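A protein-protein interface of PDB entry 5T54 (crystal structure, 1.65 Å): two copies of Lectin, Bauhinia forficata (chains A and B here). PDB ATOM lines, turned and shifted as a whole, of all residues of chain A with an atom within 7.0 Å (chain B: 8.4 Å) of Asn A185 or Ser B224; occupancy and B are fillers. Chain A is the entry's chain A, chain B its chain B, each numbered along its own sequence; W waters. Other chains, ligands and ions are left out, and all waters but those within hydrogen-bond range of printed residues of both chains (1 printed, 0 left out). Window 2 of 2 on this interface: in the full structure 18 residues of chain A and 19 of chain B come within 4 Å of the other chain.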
ATOM      1  N   ARG A 149       0.175  29.083  -0.723  1.00  0.00           N
ATOM      2  CA  ARG A 149      -0.737  30.200  -0.961  1.00  0.00           C
ATOM      3  C   ARG A 149      -2.049  29.996  -0.229  1.00  0.00           C
ATOM      4  O   ARG A 149      -2.621  28.908  -0.240  1.00  0.00           O
ATOM      5  CB  ARG A 149      -1.029  30.315  -2.444  1.00  0.00           C
ATOM      6  CG  ARG A 149      -1.849  31.518  -2.758  1.00  0.00           C
ATOM      7  CD  ARG A 149      -1.845  31.727  -4.280  1.00  0.00           C
ATOM      8  NE  ARG A 149      -2.306  33.069  -4.474  1.00  0.00           N
ATOM      9  CZ  ARG A 149      -1.679  33.999  -5.178  1.00  0.00           C
ATOM     10  NH1 ARG A 149      -0.553  33.739  -5.829  1.00  0.00           N
ATOM     11  NH2 ARG A 149      -2.220  35.190  -5.271  1.00  0.00           N
ATOM     12  N   ASP A 154     -10.742  32.816   0.669  1.00  0.00           N
ATOM     13  CA  ASP A 154     -10.856  32.178   1.962  1.00  0.00           C
ATOM     14  C   ASP A 154     -10.448  33.158   3.112  1.00  0.00           C
ATOM     15  O   ASP A 154     -11.151  33.242   4.117  1.00  0.00           O
ATOM     16  CB  ASP A 154     -10.014  30.879   2.064  1.00  0.00           C
ATOM     17  CG  ASP A 154     -10.511  29.751   1.111  1.00  0.00           C
ATOM     18  OD1 ASP A 154     -11.716  29.591   0.971  1.00  0.00           O
ATOM     19  OD2 ASP A 154      -9.641  29.075   0.430  1.00  0.00           O
ATOM     20  N   PHE A 177      -3.891  20.245   7.900  1.00  0.00           N
ATOM     21  CA  PHE A 177      -4.953  20.326   6.935  1.00  0.00           C
ATOM     22  C   PHE A 177      -5.879  21.436   7.379  1.00  0.00           C
ATOM     23  O   PHE A 177      -6.338  21.499   8.531  1.00  0.00           O
ATOM     24  CB  PHE A 177      -5.810  19.048   6.869  1.00  0.00           C
ATOM     25  CG  PHE A 177      -5.067  17.732   6.608  1.00  0.00           C
ATOM     26  CD1 PHE A 177      -3.958  17.650   5.819  1.00  0.00           C
ATOM     27  CD2 PHE A 177      -5.610  16.554   7.136  1.00  0.00           C
ATOM     28  CE1 PHE A 177      -3.365  16.431   5.577  1.00  0.00           C
ATOM     29  CE2 PHE A 177      -5.026  15.320   6.875  1.00  0.00           C
ATOM     30  CZ  PHE A 177      -3.894  15.266   6.070  1.00  0.00           C
ATOM     31  N   VAL A 178      -6.091  22.365   6.480  1.00  0.00           N
ATOM     32  CA  VAL A 178      -7.005  23.501   6.790  1.00  0.00           C
ATOM     33  C   VAL A 178      -8.156  23.461   5.785  1.00  0.00           C
ATOM     34  O   VAL A 178      -7.941  23.332   4.555  1.00  0.00           O
ATOM     35  CB  VAL A 178      -6.211  24.844   6.721  1.00  0.00           C
ATOM     36  CG1 VAL A 178      -7.109  26.064   6.929  1.00  0.00           C
ATOM     37  CG2 VAL A 178      -5.081  24.884   7.730  1.00  0.00           C
ATOM     38  N   THR A 179      -9.377  23.576   6.259  1.00  0.00           N
ATOM     39  CA  THR A 179     -10.536  23.524   5.361  1.00  0.00           C
ATOM     40  C   THR A 179     -11.484  24.695   5.584  1.00  0.00           C
ATOM     41  O   THR A 179     -11.649  25.163   6.759  1.00  0.00           O
ATOM     42  CB  THR A 179     -11.352  22.202   5.560  1.00  0.00           C
ATOM     43  OG1 THR A 179     -11.932  22.182   6.885  1.00  0.00           O
ATOM     44  CG2 THR A 179     -10.467  20.975   5.495  1.00  0.00           C
ATOM     45  N   TYR A 180     -12.148  25.103   4.492  1.00  0.00           N
ATOM     46  CA  TYR A 180     -13.143  26.163   4.521  1.00  0.00           C
ATOM     47  C   TYR A 180     -14.413  25.609   4.005  1.00  0.00           C
ATOM     48  O   TYR A 180     -14.370  24.883   2.997  1.00  0.00           O
ATOM     49  CB  TYR A 180     -12.701  27.361   3.629  1.00  0.00           C
ATOM     50  CG  TYR A 180     -11.684  28.263   4.317  1.00  0.00           C
ATOM     51  CD1 TYR A 180     -10.335  27.926   4.436  1.00  0.00           C
ATOM     52  CD2 TYR A 180     -12.110  29.460   4.907  1.00  0.00           C
ATOM     53  CE1 TYR A 180      -9.430  28.722   5.084  1.00  0.00           C
ATOM     54  CE2 TYR A 180     -11.185  30.273   5.540  1.00  0.00           C
ATOM     55  CZ  TYR A 180      -9.863  29.910   5.670  1.00  0.00           C
ATOM     56  OH  TYR A 180      -8.932  30.731   6.333  1.00  0.00           O
ATOM     57  N   PRO A 181     -15.534  25.956   4.640  1.00  0.00           N
ATOM     58  CA  PRO A 181     -16.835  25.450   4.150  1.00  0.00           C
ATOM     59  C   PRO A 181     -17.154  25.979   2.798  1.00  0.00           C
ATOM     60  O   PRO A 181     -17.074  27.164   2.533  1.00  0.00           O
ATOM     61  CB  PRO A 181     -17.835  25.816   5.261  1.00  0.00           C
ATOM     62  CG  PRO A 181     -17.207  26.940   5.950  1.00  0.00           C
ATOM     63  CD  PRO A 181     -15.692  26.798   5.874  1.00  0.00           C
ATOM     64  N   GLY A 183     -15.149  26.158   0.438  1.00  0.00           N
ATOM     65  CA  GLY A 183     -13.998  26.943   0.102  1.00  0.00           C
ATOM     66  C   GLY A 183     -12.789  26.023  -0.117  1.00  0.00           C
ATOM     67  O   GLY A 183     -12.874  24.803  -0.399  1.00  0.00           O
ATOM     68  N   GLY A 184     -11.621  26.606   0.006  1.00  0.00           N
ATOM     69  CA  GLY A 184     -10.407  25.886  -0.238  1.00  0.00           C
ATOM     70  C   GLY A 184      -9.995  24.924   0.820  1.00  0.00           C
ATOM     71  O   GLY A 184     -10.454  25.019   1.990  1.00  0.00           O
ATOM     72  N   ASN A 185      -9.079  24.018   0.438  1.00  0.00           N
ATOM     73  CA  ASN A 185      -8.478  23.054   1.361  1.00  0.00           C
ATOM     74  C   ASN A 185      -7.025  23.184   1.169  1.00  0.00           C
ATOM     75  O   ASN A 185      -6.516  23.418   0.040  1.00  0.00           O
ATOM     76  CB  ASN A 185      -8.943  21.582   1.173  1.00  0.00           C
ATOM     77  CG  ASN A 185     -10.458  21.432   1.289  1.00  0.00           C
ATOM     78  OD1 ASN A 185     -11.079  21.859   2.268  1.00  0.00           O
ATOM     79  ND2 ASN A 185     -11.043  20.775   0.309  1.00  0.00           N
ATOM     80  N   TYR A 186      -6.298  23.072   2.271  1.00  0.00           N
ATOM     81  CA  TYR A 186      -4.889  23.283   2.317  1.00  0.00           C
ATOM     82  C   TYR A 186      -4.177  22.134   3.022  1.00  0.00           C
ATOM     83  O   TYR A 186      -4.608  21.729   4.088  1.00  0.00           O
ATOM     84  CB  TYR A 186      -4.498  24.590   3.047  1.00  0.00           C
ATOM     85  CG  TYR A 186      -5.182  25.794   2.431  1.00  0.00           C
ATOM     86  CD1 TYR A 186      -6.488  26.133   2.781  1.00  0.00           C
ATOM     87  CD2 TYR A 186      -4.538  26.542   1.374  1.00  0.00           C
ATOM     88  CE1 TYR A 186      -7.126  27.208   2.167  1.00  0.00           C
ATOM     89  CE2 TYR A 186      -5.201  27.580   0.717  1.00  0.00           C
ATOM     90  CZ  TYR A 186      -6.450  27.929   1.163  1.00  0.00           C
ATOM     91  OH  TYR A 186      -7.083  29.023   0.524  1.00  0.00           O
ATOM     92  N   VAL A 187      -3.048  21.684   2.457  1.00  0.00           N
ATOM     93  CA  VAL A 187      -2.253  20.586   3.013  1.00  0.00           C
ATOM     94  C   VAL A 187      -0.750  20.943   3.081  1.00  0.00           C
ATOM     95  O   VAL A 187      -0.142  21.249   2.015  1.00  0.00           O
ATOM     96  CB  VAL A 187      -2.400  19.313   2.120  1.00  0.00           C
ATOM     97  CG1 VAL A 187      -1.499  18.190   2.606  1.00  0.00           C
ATOM     98  CG2 VAL A 187      -3.868  18.856   2.108  1.00  0.00           C
ATOM     99  N   SER B   1      -2.880  17.399 -11.354  1.00  0.00           N
ATOM    100  CA  SER B   1      -3.949  18.188 -11.990  1.00  0.00           C
ATOM    101  C   SER B   1      -5.012  18.491 -10.957  1.00  0.00           C
ATOM    102  O   SER B   1      -5.034  17.927  -9.818  1.00  0.00           O
ATOM    103  CB  SER B   1      -4.531  17.370 -13.164  1.00  0.00           C
ATOM    104  OG  SER B   1      -5.155  16.202 -12.620  1.00  0.00           O
ATOM    105  N   GLU B   2      -5.938  19.341 -11.367  1.00  0.00           N
ATOM    106  CA  GLU B   2      -7.012  19.842 -10.510  1.00  0.00           C
ATOM    107  C   GLU B   2      -8.358  19.114 -10.703  1.00  0.00           C
ATOM    108  O   GLU B   2      -8.827  18.973 -11.808  1.00  0.00           O
ATOM    109  CB  GLU B   2      -7.072  21.360 -10.705  1.00  0.00           C
ATOM    110  CG  GLU B   2      -5.636  21.945 -10.375  1.00  0.00           C
ATOM    111  CD  GLU B   2      -5.618  23.371  -9.839  1.00  0.00           C
ATOM    112  OE1 GLU B   2      -6.687  24.027  -9.881  1.00  0.00           O
ATOM    113  OE2 GLU B   2      -4.565  23.861  -9.364  1.00  0.00           O
ATOM    114  N   LEU B   3      -8.942  18.602  -9.601  1.00  0.00           N
ATOM    115  CA  LEU B   3     -10.196  17.880  -9.597  1.00  0.00           C
ATOM    116  C   LEU B   3     -10.841  18.109  -8.249  1.00  0.00           C
ATOM    117  O   LEU B   3     -10.151  18.096  -7.234  1.00  0.00           O
ATOM    118  CB  LEU B   3      -9.920  16.377  -9.800  1.00  0.00           C
ATOM    119  CG  LEU B   3     -11.053  15.403  -9.529  1.00  0.00           C
ATOM    120  CD1 LEU B   3     -12.137  15.565 -10.615  1.00  0.00           C
ATOM    121  CD2 LEU B   3     -10.501  14.010  -9.518  1.00  0.00           C
ATOM    122  N   SER B   4     -12.143  18.298  -8.217  1.00  0.00           N
ATOM    123  CA  SER B   4     -12.821  18.279  -6.918  1.00  0.00           C
ATOM    124  C   SER B   4     -14.191  17.621  -7.045  1.00  0.00           C
ATOM    125  O   SER B   4     -14.826  17.657  -8.065  1.00  0.00           O
ATOM    126  CB  SER B   4     -12.866  19.667  -6.250  1.00  0.00           C
ATOM    127  OG  SER B   4     -13.899  20.331  -6.814  1.00  0.00           O
ATOM    128  N   PHE B   5     -14.612  16.948  -5.999  1.00  0.00           N
ATOM    129  CA  PHE B   5     -15.910  16.361  -5.934  1.00  0.00           C
ATOM    130  C   PHE B   5     -16.374  16.282  -4.470  1.00  0.00           C
ATOM    131  O   PHE B   5     -15.581  16.398  -3.519  1.00  0.00           O
ATOM    132  CB  PHE B   5     -15.964  14.999  -6.634  1.00  0.00           C
ATOM    133  CG  PHE B   5     -15.017  13.921  -6.080  1.00  0.00           C
ATOM    134  CD1 PHE B   5     -15.358  13.201  -4.936  1.00  0.00           C
ATOM    135  CD2 PHE B   5     -13.810  13.599  -6.752  1.00  0.00           C
ATOM    136  CE1 PHE B   5     -14.481  12.172  -4.477  1.00  0.00           C
ATOM    137  CE2 PHE B   5     -12.944  12.612  -6.291  1.00  0.00           C
ATOM    138  CZ  PHE B   5     -13.317  11.884  -5.151  1.00  0.00           C
ATOM    139  N   ASN B   6     -17.674  16.141  -4.332  1.00  0.00           N
ATOM    140  CA  ASN B   6     -18.338  16.182  -3.053  1.00  0.00           C
ATOM    141  C   ASN B   6     -19.641  15.342  -2.990  1.00  0.00           C
ATOM    142  O   ASN B   6     -20.609  15.589  -3.712  1.00  0.00           O
ATOM    143  CB  ASN B   6     -18.619  17.633  -2.708  1.00  0.00           C
ATOM    144  CG  ASN B   6     -19.303  17.789  -1.378  1.00  0.00           C
ATOM    145  OD1 ASN B   6     -19.204  16.987  -0.488  1.00  0.00           O
ATOM    146  ND2 ASN B   6     -20.083  18.878  -1.267  1.00  0.00           N
ATOM    147  N   PHE B  54      -7.108  11.683 -12.457  1.00  0.00           N
ATOM    148  CA  PHE B  54      -6.336  12.878 -12.203  1.00  0.00           C
ATOM    149  C   PHE B  54      -4.854  12.484 -12.269  1.00  0.00           C
ATOM    150  O   PHE B  54      -4.540  11.305 -12.464  1.00  0.00           O
ATOM    151  CB  PHE B  54      -6.698  13.558 -10.881  1.00  0.00           C
ATOM    152  CG  PHE B  54      -6.450  12.752  -9.654  1.00  0.00           C
ATOM    153  CD1 PHE B  54      -7.393  11.793  -9.256  1.00  0.00           C
ATOM    154  CD2 PHE B  54      -5.351  12.979  -8.870  1.00  0.00           C
ATOM    155  CE1 PHE B  54      -7.211  11.074  -8.105  1.00  0.00           C
ATOM    156  CE2 PHE B  54      -5.137  12.231  -7.705  1.00  0.00           C
ATOM    157  CZ  PHE B  54      -6.076  11.274  -7.333  1.00  0.00           C
ATOM    158  N   THR B  59       1.198  18.068  -7.760  1.00  0.00           N
ATOM    159  CA  THR B  59      -0.171  18.111  -7.238  1.00  0.00           C
ATOM    160  C   THR B  59      -0.184  17.786  -5.759  1.00  0.00           C
ATOM    161  O   THR B  59       0.580  16.912  -5.293  1.00  0.00           O
ATOM    162  CB  THR B  59      -1.003  17.028  -7.970  1.00  0.00           C
ATOM    163  OG1 THR B  59      -1.005  17.386  -9.367  1.00  0.00           O
ATOM    164  CG2 THR B  59      -2.439  16.901  -7.421  1.00  0.00           C
ATOM    165  N   SER B  60      -1.011  18.520  -5.017  1.00  0.00           N
ATOM    166  CA  SER B  60      -1.359  18.107  -3.716  1.00  0.00           C
ATOM    167  C   SER B  60      -2.811  17.752  -3.696  1.00  0.00           C
ATOM    168  O   SER B  60      -3.610  18.244  -4.495  1.00  0.00           O
ATOM    169  CB  SER B  60      -1.113  19.266  -2.660  1.00  0.00           C
ATOM    170  OG  SER B  60       0.233  19.570  -2.490  1.00  0.00           O
ATOM    171  N   PHE B  61      -3.266  16.939  -2.708  1.00  0.00           N
ATOM    172  CA  PHE B  61      -4.687  16.673  -2.579  1.00  0.00           C
ATOM    173  C   PHE B  61      -5.123  16.507  -1.113  1.00  0.00           C
ATOM    174  O   PHE B  61      -4.332  16.201  -0.198  1.00  0.00           O
ATOM    175  CB  PHE B  61      -5.184  15.443  -3.432  1.00  0.00           C
ATOM    176  CG  PHE B  61      -4.696  14.092  -2.955  1.00  0.00           C
ATOM    177  CD1 PHE B  61      -5.237  13.490  -1.875  1.00  0.00           C
ATOM    178  CD2 PHE B  61      -3.680  13.427  -3.667  1.00  0.00           C
ATOM    179  CE1 PHE B  61      -4.749  12.221  -1.448  1.00  0.00           C
ATOM    180  CE2 PHE B  61      -3.236  12.139  -3.286  1.00  0.00           C
ATOM    181  CZ  PHE B  61      -3.759  11.585  -2.159  1.00  0.00           C
ATOM    182  N   TYR B  62      -6.384  16.778  -0.932  1.00  0.00           N
ATOM    183  CA  TYR B  62      -7.050  16.563   0.395  1.00  0.00           C
ATOM    184  C   TYR B  62      -8.308  15.762   0.171  1.00  0.00           C
ATOM    185  O   TYR B  62      -9.117  16.087  -0.731  1.00  0.00           O
ATOM    186  CB  TYR B  62      -7.364  17.891   1.115  1.00  0.00           C
ATOM    187  CG  TYR B  62      -8.245  17.702   2.300  1.00  0.00           C
ATOM    188  CD1 TYR B  62      -7.717  17.337   3.504  1.00  0.00           C
ATOM    189  CD2 TYR B  62      -9.638  17.948   2.240  1.00  0.00           C
ATOM    190  CE1 TYR B  62      -8.520  17.108   4.621  1.00  0.00           C
ATOM    191  CE2 TYR B  62     -10.450  17.761   3.346  1.00  0.00           C
ATOM    192  CZ  TYR B  62      -9.917  17.323   4.541  1.00  0.00           C
ATOM    193  OH  TYR B  62     -10.686  17.187   5.719  1.00  0.00           O
ATOM    194  N   THR B  63      -8.550  14.732   0.969  1.00  0.00           N
ATOM    195  CA  THR B  63      -9.825  14.021   0.890  1.00  0.00           C
ATOM    196  C   THR B  63     -10.332  13.608   2.264  1.00  0.00           C
ATOM    197  O   THR B  63      -9.520  13.405   3.162  1.00  0.00           O
ATOM    198  CB  THR B  63      -9.681  12.806  -0.085  1.00  0.00           C
ATOM    199  OG1 THR B  63     -10.956  12.182  -0.354  1.00  0.00           O
ATOM    200  CG2 THR B  63      -8.822  11.697   0.506  1.00  0.00           C
ATOM    201  N   THR B  64     -11.647  13.615   2.451  1.00  0.00           N
ATOM    202  CA  THR B  64     -12.222  13.170   3.722  1.00  0.00           C
ATOM    203  C   THR B  64     -13.416  12.306   3.432  1.00  0.00           C
ATOM    204  O   THR B  64     -14.139  12.524   2.469  1.00  0.00           O
ATOM    205  CB  THR B  64     -12.514  14.364   4.639  1.00  0.00           C
ATOM    206  OG1 THR B  64     -12.996  13.888   5.913  1.00  0.00           O
ATOM    207  CG2 THR B  64     -13.573  15.238   4.044  1.00  0.00           C
ATOM    208  N   VAL B 165      -7.348  12.282   4.571  1.00  0.00           N
ATOM    209  CA  VAL B 165      -6.094  11.837   3.965  1.00  0.00           C
ATOM    210  C   VAL B 165      -5.609  12.945   3.082  1.00  0.00           C
ATOM    211  O   VAL B 165      -6.332  13.490   2.251  1.00  0.00           O
ATOM    212  CB  VAL B 165      -6.324  10.548   3.162  1.00  0.00           C
ATOM    213  CG1 VAL B 165      -5.094  10.141   2.342  1.00  0.00           C
ATOM    214  CG2 VAL B 165      -6.833   9.440   4.109  1.00  0.00           C
ATOM    215  N   GLY B 166      -4.363  13.318   3.248  1.00  0.00           N
ATOM    216  CA  GLY B 166      -3.760  14.415   2.533  1.00  0.00           C
ATOM    217  C   GLY B 166      -2.437  14.036   1.950  1.00  0.00           C
ATOM    218  O   GLY B 166      -1.649  13.279   2.540  1.00  0.00           O
ATOM    219  N   TYR B 167      -2.118  14.631   0.805  1.00  0.00           N
ATOM    220  CA  TYR B 167      -0.808  14.474   0.154  1.00  0.00           C
ATOM    221  C   TYR B 167      -0.258  15.857  -0.177  1.00  0.00           C
ATOM    222  O   TYR B 167      -0.873  16.650  -0.923  1.00  0.00           O
ATOM    223  CB  TYR B 167      -0.906  13.652  -1.130  1.00  0.00           C
ATOM    224  CG  TYR B 167       0.431  13.447  -1.807  1.00  0.00           C
ATOM    225  CD1 TYR B 167       1.453  12.676  -1.192  1.00  0.00           C
ATOM    226  CD2 TYR B 167       0.764  14.075  -3.011  1.00  0.00           C
ATOM    227  CE1 TYR B 167       2.643  12.527  -1.806  1.00  0.00           C
ATOM    228  CE2 TYR B 167       1.983  13.884  -3.610  1.00  0.00           C
ATOM    229  CZ  TYR B 167       2.912  13.114  -3.006  1.00  0.00           C
ATOM    230  OH  TYR B 167       4.143  12.915  -3.654  1.00  0.00           O
ATOM    231  N   ILE B 204      -8.877   7.481  -7.643  1.00  0.00           N
ATOM    232  CA  ILE B 204      -9.038   7.255  -6.180  1.00  0.00           C
ATOM    233  C   ILE B 204     -10.361   6.546  -5.818  1.00  0.00           C
ATOM    234  O   ILE B 204     -11.412   6.840  -6.437  1.00  0.00           O
ATOM    235  CB  ILE B 204      -8.844   8.604  -5.401  1.00  0.00           C
ATOM    236  CG1 ILE B 204      -8.650   8.336  -3.920  1.00  0.00           C
ATOM    237  CG2 ILE B 204     -10.013   9.600  -5.631  1.00  0.00           C
ATOM    238  CD1 ILE B 204      -8.182   9.501  -3.127  1.00  0.00           C
ATOM    239  N   TRP B 221     -18.162  11.577   1.289  1.00  0.00           N
ATOM    240  CA  TRP B 221     -16.863  11.669   0.705  1.00  0.00           C
ATOM    241  C   TRP B 221     -16.665  12.910  -0.135  1.00  0.00           C
ATOM    242  O   TRP B 221     -17.514  13.229  -0.957  1.00  0.00           O
ATOM    243  CB  TRP B 221     -16.627  10.484  -0.270  1.00  0.00           C
ATOM    244  CG  TRP B 221     -15.205  10.272  -0.817  1.00  0.00           C
ATOM    245  CD1 TRP B 221     -13.982  10.646  -0.276  1.00  0.00           C
ATOM    246  CD2 TRP B 221     -14.890   9.563  -2.033  1.00  0.00           C
ATOM    247  NE1 TRP B 221     -12.942  10.235  -1.085  1.00  0.00           N
ATOM    248  CE2 TRP B 221     -13.488   9.482  -2.113  1.00  0.00           C
ATOM    249  CE3 TRP B 221     -15.681   8.918  -3.013  1.00  0.00           C
ATOM    250  CZ2 TRP B 221     -12.838   8.881  -3.176  1.00  0.00           C
ATOM    251  CZ3 TRP B 221     -15.006   8.245  -4.051  1.00  0.00           C
ATOM    252  CH2 TRP B 221     -13.618   8.219  -4.101  1.00  0.00           C
ATOM    253  N   SER B 222     -15.578  13.610   0.130  1.00  0.00           N
ATOM    254  CA  SER B 222     -15.165  14.759  -0.655  1.00  0.00           C
ATOM    255  C   SER B 222     -13.669  14.789  -0.933  1.00  0.00           C
ATOM    256  O   SER B 222     -12.910  14.144  -0.240  1.00  0.00           O
ATOM    257  CB  SER B 222     -15.652  16.069  -0.088  1.00  0.00           C
ATOM    258  OG  SER B 222     -14.980  16.363   1.162  1.00  0.00           O
ATOM    259  N   PHE B 223     -13.265  15.508  -1.972  1.00  0.00           N
ATOM    260  CA  PHE B 223     -11.903  15.473  -2.519  1.00  0.00           C
ATOM    261  C   PHE B 223     -11.612  16.758  -3.259  1.00  0.00           C
ATOM    262  O   PHE B 223     -12.459  17.299  -3.951  1.00  0.00           O
ATOM    263  CB  PHE B 223     -11.743  14.326  -3.557  1.00  0.00           C
ATOM    264  CG  PHE B 223     -10.397  14.235  -4.229  1.00  0.00           C
ATOM    265  CD1 PHE B 223     -10.076  14.983  -5.398  1.00  0.00           C
ATOM    266  CD2 PHE B 223      -9.451  13.307  -3.821  1.00  0.00           C
ATOM    267  CE1 PHE B 223      -8.896  14.874  -6.044  1.00  0.00           C
ATOM    268  CE2 PHE B 223      -8.250  13.201  -4.490  1.00  0.00           C
ATOM    269  CZ  PHE B 223      -7.947  13.972  -5.543  1.00  0.00           C
ATOM    270  N   SER B 224     -10.432  17.278  -3.056  1.00  0.00           N
ATOM    271  CA  SER B 224      -9.910  18.400  -3.907  1.00  0.00           C
ATOM    272  C   SER B 224      -8.409  18.157  -4.140  1.00  0.00           C
ATOM    273  O   SER B 224      -7.679  17.768  -3.249  1.00  0.00           O
ATOM    274  CB  SER B 224     -10.187  19.750  -3.308  1.00  0.00           C
ATOM    275  OG  SER B 224      -9.625  19.840  -2.007  1.00  0.00           O
ATOM    276  N   SER B 225      -7.952  18.436  -5.366  1.00  0.00           N
ATOM    277  CA  SER B 225      -6.564  18.396  -5.755  1.00  0.00           C
ATOM    278  C   SER B 225      -6.257  19.742  -6.396  1.00  0.00           C
ATOM    279  O   SER B 225      -7.151  20.339  -7.045  1.00  0.00           O
ATOM    280  CB  SER B 225      -6.200  17.253  -6.739  1.00  0.00           C
ATOM    281  OG  SER B 225      -6.902  17.302  -7.968  1.00  0.00           O
ATOM    282  N   THR B 226      -5.063  20.223  -6.143  1.00  0.00           N
ATOM    283  CA  THR B 226      -4.557  21.484  -6.734  1.00  0.00           C
ATOM    284  C   THR B 226      -3.098  21.353  -7.157  1.00  0.00           C
ATOM    285  O   THR B 226      -2.336  20.560  -6.663  1.00  0.00           O
ATOM    286  CB  THR B 226      -4.623  22.672  -5.760  1.00  0.00           C
ATOM    287  OG1 THR B 226      -3.737  22.439  -4.671  1.00  0.00           O
ATOM    288  CG2 THR B 226      -5.969  22.830  -5.190  1.00  0.00           C
ATOM    289  N   SER B 227      -2.717  22.238  -8.065  1.00  0.00           N
ATOM    290  CA  SER B 227      -1.359  22.269  -8.583  1.00  0.00           C
ATOM    291  C   SER B 227      -0.468  22.868  -7.532  1.00  0.00           C
ATOM    292  O   SER B 227      -0.848  23.804  -6.818  1.00  0.00           O
ATOM    293  CB  SER B 227      -1.312  23.163  -9.817  1.00  0.00           C
ATOM    294  OG  SER B 227      -0.024  23.128 -10.396  1.00  0.00           O
HETATM  295  O   HOH W   1       0.142  21.496  -0.607  1.00  0.00           O
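N of Tyr B62 is in hydrogen-bond range of O of Ser B224.
O of Tyr B167 sits close to OG of Ser B60.
The backbone carbonyl oxygen of Phe B61 lies within hydrogen-bond range of the backbone NH of Tyr B167, at 2.9 Å.
Tyr B62 touches Phe A177 (CE1 to CD2, 3.9 Å).
Phe A177 touches Gly B166.
OH of Tyr B62 touches CG2 of Thr A179, at 3.8 Å.
Asn A185 touches Tyr B62.
Phe B61 touches Val A187 (O to CG2, 3.5 Å).
CG2 of Val A187 touches CB of Tyr B62, 3.8 Å away.
Tyr B167 touches Val A187.
Water W1 bridges O of Val A187 (2.6 Å) and OG of Ser B60 (2.7 Å).
The side-chain hydroxyl (OG) of Ser B224 lies within hydrogen-bond range of the side-chain amide nitrogen (ND2) of Asn A185 (2.9 Å).
No position is printed for both chains.
Of the 8 pairs that touch across the chains among the printed residues, none has its exchanged pair printed and touching as well.
Printed residues of chain B within 4 Å of Phe A177: Tyr B62 and Gly B166.
Gly A184 touches none of the printed residues of chain B.
Printed residues of chain B within 4 Å of Asn A185: Tyr B62 (3.7 Å) and Ser B224 (2.9 Å).
Ser B4 touches none of the printed residues of chain A.
Of the printed residues of chain A, Tyr B62 touches Phe A177 (3.9 Å), Thr A179 (3.8 Å), Asn A185 (3.7 Å) and Val A187 (3.8 Å).
Of the printed residues of chain A, Gly B166 touches Phe A177.
Of the printed residues of chain A, Tyr B167 touches Val A187.
Ser B224 touches one residue of chain A.
The nearest printed residue of chain B that does not touch Phe A177 is Val B165 (4.2 Å).
Hydrophobic or aromatic side chains of chain B that line the printed part of chain A: Tyr B62.
Of the 12 printed residues of chain A, 4 touch a printed residue of chain B.
Printed residues of chain A that touch a printed residue of chain B: Phe A177, Thr A179, Asn A185 and Val A187.
Hydrophobic or aromatic side chains of chain A that line the printed part of chain B: Phe A177 and Val A187.
Among the printed residues, no Asp or Glu carboxylate lies within 4 Å of a Lys or Arg side-chain nitrogen of the other chain.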
